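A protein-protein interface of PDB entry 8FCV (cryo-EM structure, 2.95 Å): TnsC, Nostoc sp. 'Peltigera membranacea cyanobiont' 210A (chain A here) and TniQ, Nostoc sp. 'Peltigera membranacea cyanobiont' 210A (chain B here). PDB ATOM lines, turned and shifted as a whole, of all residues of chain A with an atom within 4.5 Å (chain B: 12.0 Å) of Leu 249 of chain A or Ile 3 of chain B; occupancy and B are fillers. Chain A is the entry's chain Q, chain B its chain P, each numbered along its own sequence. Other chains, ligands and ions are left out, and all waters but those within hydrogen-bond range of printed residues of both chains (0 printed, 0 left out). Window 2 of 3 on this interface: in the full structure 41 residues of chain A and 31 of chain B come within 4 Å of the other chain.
Thr 5 of chain A touches one residue of chain B.
Of chain B, only Ile 3 (3.5 Å) and Tyr 4 (3.1 Å) come within 4 Å of Ser 246 of chain A.
Of the printed residues of chain B, Val 247 of chain A touches Tyr 4 (3.6 Å).
No residue of chain B comes within 4 Å of Leu 248 of chain A.
Leu 249 of chain A touches just one residue of chain B: Ile 3.
Of chain B, only Ile 3 and Tyr 4 come within 4 Å of Thr 250 of chain A.
No residue of chain B comes within 4 Å of Gln 252 of chain A.
Gln 253 of chain A touches just one residue of chain B: Ile 3 (3.3 Å).
No residue of chain B comes within 4 Å of Val 264 of chain A.
Printed residues of chain A within 4 Å of Tyr 4 of chain B: Ser 246, Val 247 and Thr 250.
NE2 of Gln 253 of chain A is in hydrogen-bond range of OG1 of Thr 5 of chain A, 3.1 Å away.
The backbone carbonyl oxygen (O) of Leu 249 of chain A lies close to the side-chain amide oxygen (OE1) of Gln 253 of chain A (3.3 Å).
Hydrophobic or aromatic side chains of chain B within 4 Å of the printed part of chain A: Ile 3 and Tyr 4.
Of the 11 printed residues of chain A, 6 touch a printed residue of chain B.
Along chain A the printed residues that touch a printed residue of chain B span positions 5 to 253.
Among the printed residues, pairs that only touch across the chains: Thr 5 of chain A with Ile 3 of chain B (3.6 Å), Ser 246 of chain A with Ile 3 of chain B (3.5 Å), Ser 246 of chain A with Tyr 4 of chain B (3.1 Å), Val 247 of chain A with Tyr 4 of chain B (3.6 Å), Leu 249 of chain A with Ile 3 of chain B (3.7 Å), Thr 250 of chain A with Ile 3 of chain B (3.3 Å), Thr 250 of chain A with Tyr 4 of chain B (3.7 Å) and Gln 253 of chain A with Ile 3 of chain B (3.3 Å).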
ATOM      1  N   THR A   5      18.606  28.092  20.630  1.00  0.00           N
ATOM      2  CA  THR A   5      19.357  27.008  21.251  1.00  0.00           C
ATOM      3  C   THR A   5      19.431  25.766  20.375  1.00  0.00           C
ATOM      4  O   THR A   5      20.314  24.929  20.586  1.00  0.00           O
ATOM      5  CB  THR A   5      18.732  26.637  22.598  1.00  0.00           C
ATOM      6  OG1 THR A   5      17.678  25.689  22.392  1.00  0.00           O
ATOM      7  CG2 THR A   5      18.170  27.873  23.284  1.00  0.00           C
ATOM      8  N   LYS A 245      29.182  22.811  32.601  1.00  0.00           N
ATOM      9  CA  LYS A 245      27.891  22.162  32.394  1.00  0.00           C
ATOM     10  C   LYS A 245      27.065  22.902  31.349  1.00  0.00           C
ATOM     11  O   LYS A 245      26.385  22.279  30.527  1.00  0.00           O
ATOM     12  CB  LYS A 245      27.132  22.069  33.717  1.00  0.00           C
ATOM     13  CG  LYS A 245      27.699  21.040  34.681  1.00  0.00           C
ATOM     14  CD  LYS A 245      26.888  20.979  35.963  1.00  0.00           C
ATOM     15  CE  LYS A 245      27.455  19.946  36.922  1.00  0.00           C
ATOM     16  NZ  LYS A 245      26.754  19.959  38.235  1.00  0.00           N
ATOM     17  N   SER A 246      27.115  24.235  31.366  1.00  0.00           N
ATOM     18  CA  SER A 246      26.351  25.020  30.402  1.00  0.00           C
ATOM     19  C   SER A 246      26.881  24.832  28.983  1.00  0.00           C
ATOM     20  O   SER A 246      26.096  24.749  28.030  1.00  0.00           O
ATOM     21  CB  SER A 246      26.373  26.496  30.794  1.00  0.00           C
ATOM     22  OG  SER A 246      25.550  27.264  29.934  1.00  0.00           O
ATOM     23  N   VAL A 247      28.205  24.784  28.814  1.00  0.00           N
ATOM     24  CA  VAL A 247      28.748  24.552  27.478  1.00  0.00           C
ATOM     25  C   VAL A 247      28.433  23.135  27.013  1.00  0.00           C
ATOM     26  O   VAL A 247      28.178  22.905  25.827  1.00  0.00           O
ATOM     27  CB  VAL A 247      30.257  24.866  27.413  1.00  0.00           C
ATOM     28  CG1 VAL A 247      30.544  26.244  27.991  1.00  0.00           C
ATOM     29  CG2 VAL A 247      31.086  23.804  28.107  1.00  0.00           C
ATOM     30  N   LEU A 248      28.414  22.167  27.936  1.00  0.00           N
ATOM     31  CA  LEU A 248      27.951  20.831  27.570  1.00  0.00           C
ATOM     32  C   LEU A 248      26.500  20.862  27.106  1.00  0.00           C
ATOM     33  O   LEU A 248      26.143  20.225  26.108  1.00  0.00           O
ATOM     34  CB  LEU A 248      28.106  19.873  28.752  1.00  0.00           C
ATOM     35  CG  LEU A 248      29.365  19.010  28.790  1.00  0.00           C
ATOM     36  CD1 LEU A 248      29.349  18.116  30.016  1.00  0.00           C
ATOM     37  CD2 LEU A 248      29.476  18.179  27.524  1.00  0.00           C
ATOM     38  N   LEU A 249      25.652  21.608  27.818  1.00  0.00           N
ATOM     39  CA  LEU A 249      24.243  21.694  27.453  1.00  0.00           C
ATOM     40  C   LEU A 249      24.062  22.333  26.081  1.00  0.00           C
ATOM     41  O   LEU A 249      23.263  21.858  25.267  1.00  0.00           O
ATOM     42  CB  LEU A 249      23.480  22.482  28.517  1.00  0.00           C
ATOM     43  CG  LEU A 249      21.957  22.550  28.391  1.00  0.00           C
ATOM     44  CD1 LEU A 249      21.383  21.185  28.063  1.00  0.00           C
ATOM     45  CD2 LEU A 249      21.340  23.103  29.666  1.00  0.00           C
ATOM     46  N   THR A 250      24.800  23.411  25.804  1.00  0.00           N
ATOM     47  CA  THR A 250      24.649  24.074  24.512  1.00  0.00           C
ATOM     48  C   THR A 250      25.240  23.239  23.380  1.00  0.00           C
ATOM     49  O   THR A 250      24.718  23.265  22.260  1.00  0.00           O
ATOM     50  CB  THR A 250      25.264  25.478  24.542  1.00  0.00           C
ATOM     51  OG1 THR A 250      24.883  26.192  23.359  1.00  0.00           O
ATOM     52  CG2 THR A 250      26.778  25.424  24.614  1.00  0.00           C
ATOM     53  N   PHE A 251      26.308  22.483  23.650  1.00  0.00           N
ATOM     54  CA  PHE A 251      26.825  21.559  22.646  1.00  0.00           C
ATOM     55  C   PHE A 251      25.820  20.456  22.350  1.00  0.00           C
ATOM     56  O   PHE A 251      25.651  20.056  21.192  1.00  0.00           O
ATOM     57  CB  PHE A 251      28.156  20.970  23.110  1.00  0.00           C
ATOM     58  CG  PHE A 251      29.358  21.724  22.616  1.00  0.00           C
ATOM     59  CD1 PHE A 251      29.341  22.340  21.377  1.00  0.00           C
ATOM     60  CD2 PHE A 251      30.503  21.815  23.388  1.00  0.00           C
ATOM     61  CE1 PHE A 251      30.444  23.034  20.916  1.00  0.00           C
ATOM     62  CE2 PHE A 251      31.609  22.507  22.933  1.00  0.00           C
ATOM     63  CZ  PHE A 251      31.578  23.118  21.697  1.00  0.00           C
ATOM     64  N   GLN A 252      25.150  19.947  23.387  1.00  0.00           N
ATOM     65  CA  GLN A 252      24.108  18.946  23.176  1.00  0.00           C
ATOM     66  C   GLN A 252      22.961  19.518  22.354  1.00  0.00           C
ATOM     67  O   GLN A 252      22.477  18.881  21.410  1.00  0.00           O
ATOM     68  CB  GLN A 252      23.598  18.433  24.522  1.00  0.00           C
ATOM     69  CG  GLN A 252      22.145  17.995  24.497  1.00  0.00           C
ATOM     70  CD  GLN A 252      21.495  18.032  25.865  1.00  0.00           C
ATOM     71  OE1 GLN A 252      21.934  17.352  26.793  1.00  0.00           O
ATOM     72  NE2 GLN A 252      20.433  18.819  25.994  1.00  0.00           N
ATOM     73  N   GLN A 253      22.513  20.728  22.696  1.00  0.00           N
ATOM     74  CA  GLN A 253      21.404  21.341  21.978  1.00  0.00           C
ATOM     75  C   GLN A 253      21.781  21.750  20.560  1.00  0.00           C
ATOM     76  O   GLN A 253      20.891  21.912  19.719  1.00  0.00           O
ATOM     77  CB  GLN A 253      20.881  22.554  22.750  1.00  0.00           C
ATOM     78  CG  GLN A 253      20.200  22.203  24.063  1.00  0.00           C
ATOM     79  CD  GLN A 253      19.858  23.427  24.888  1.00  0.00           C
ATOM     80  OE1 GLN A 253      20.692  23.942  25.631  1.00  0.00           O
ATOM     81  NE2 GLN A 253      18.623  23.900  24.760  1.00  0.00           N
ATOM     82  N   VAL A 264      24.656  16.315  29.696  1.00  0.00           N
ATOM     83  CA  VAL A 264      25.014  17.017  30.925  1.00  0.00           C
ATOM     84  C   VAL A 264      25.216  16.044  32.081  1.00  0.00           C
ATOM     85  O   VAL A 264      25.970  16.334  33.017  1.00  0.00           O
ATOM     86  CB  VAL A 264      23.948  18.076  31.260  1.00  0.00           C
ATOM     87  CG1 VAL A 264      24.515  19.118  32.211  1.00  0.00           C
ATOM     88  CG2 VAL A 264      23.436  18.731  29.987  1.00  0.00           C
ATOM     89  N   ILE B   3      21.840  28.668  28.546  1.00  0.00           N
ATOM     90  CA  ILE B   3      23.068  28.470  27.789  1.00  0.00           C
ATOM     91  C   ILE B   3      23.495  29.774  27.127  1.00  0.00           C
ATOM     92  O   ILE B   3      22.967  30.841  27.439  1.00  0.00           O
ATOM     93  CB  ILE B   3      22.902  27.358  26.743  1.00  0.00           C
ATOM     94  CG1 ILE B   3      21.872  27.765  25.687  1.00  0.00           C
ATOM     95  CG2 ILE B   3      22.490  26.059  27.415  1.00  0.00           C
ATOM     96  CD1 ILE B   3      21.829  26.840  24.493  1.00  0.00           C
ATOM     97  N   TYR B   4      24.457  29.684  26.211  1.00  0.00           N
ATOM     98  CA  TYR B   4      24.996  30.845  25.510  1.00  0.00           C
ATOM     99  C   TYR B   4      24.441  30.842  24.092  1.00  0.00           C
ATOM    100  O   TYR B   4      24.623  29.872  23.349  1.00  0.00           O
ATOM    101  CB  TYR B   4      26.527  30.837  25.496  1.00  0.00           C
ATOM    102  CG  TYR B   4      27.184  30.342  26.768  1.00  0.00           C
ATOM    103  CD1 TYR B   4      27.211  28.989  27.087  1.00  0.00           C
ATOM    104  CD2 TYR B   4      27.763  31.235  27.659  1.00  0.00           C
ATOM    105  CE1 TYR B   4      27.809  28.541  28.247  1.00  0.00           C
ATOM    106  CE2 TYR B   4      28.358  30.794  28.825  1.00  0.00           C
ATOM    107  CZ  TYR B   4      28.379  29.447  29.114  1.00  0.00           C
ATOM    108  OH  TYR B   4      28.972  29.005  30.273  1.00  0.00           O
ATOM    109  N   SER B   5      23.763  31.928  23.721  1.00  0.00           N
ATOM    110  CA  SER B   5      23.186  32.051  22.389  1.00  0.00           C
ATOM    111  C   SER B   5      24.162  32.617  21.366  1.00  0.00           C
ATOM    112  O   SER B   5      23.829  32.660  20.179  1.00  0.00           O
ATOM    113  CB  SER B   5      21.933  32.930  22.440  1.00  0.00           C
ATOM    114  OG  SER B   5      22.240  34.228  22.917  1.00  0.00           O
ATOM    115  N   GLU B   6      25.346  33.052  21.791  1.00  0.00           N
ATOM    116  CA  GLU B   6      26.302  33.643  20.865  1.00  0.00           C
ATOM    117  C   GLU B   6      26.934  32.564  19.992  1.00  0.00           C
ATOM    118  O   GLU B   6      27.514  31.601  20.500  1.00  0.00           O
ATOM    119  CB  GLU B   6      27.381  34.398  21.640  1.00  0.00           C
ATOM    120  CG  GLU B   6      28.295  35.253  20.779  1.00  0.00           C
ATOM    121  CD  GLU B   6      29.191  36.156  21.605  1.00  0.00           C
ATOM    122  OE1 GLU B   6      29.159  36.046  22.849  1.00  0.00           O
ATOM    123  OE2 GLU B   6      29.924  36.973  21.013  1.00  0.00           O
ATOM    124  N   HIS B   7      26.822  32.730  18.675  1.00  0.00           N
ATOM    125  CA  HIS B   7      27.399  31.795  17.709  1.00  0.00           C
ATOM    126  C   HIS B   7      28.294  32.595  16.767  1.00  0.00           C
ATOM    127  O   HIS B   7      27.800  33.309  15.888  1.00  0.00           O
ATOM    128  CB  HIS B   7      26.320  31.045  16.935  1.00  0.00           C
ATOM    129  CG  HIS B   7      25.046  31.812  16.767  1.00  0.00           C
ATOM    130  ND1 HIS B   7      24.082  31.886  17.750  1.00  0.00           N
ATOM    131  CD2 HIS B   7      24.575  32.538  15.726  1.00  0.00           C
ATOM    132  CE1 HIS B   7      23.073  32.623  17.321  1.00  0.00           C
ATOM    133  NE2 HIS B   7      23.348  33.034  16.096  1.00  0.00           N
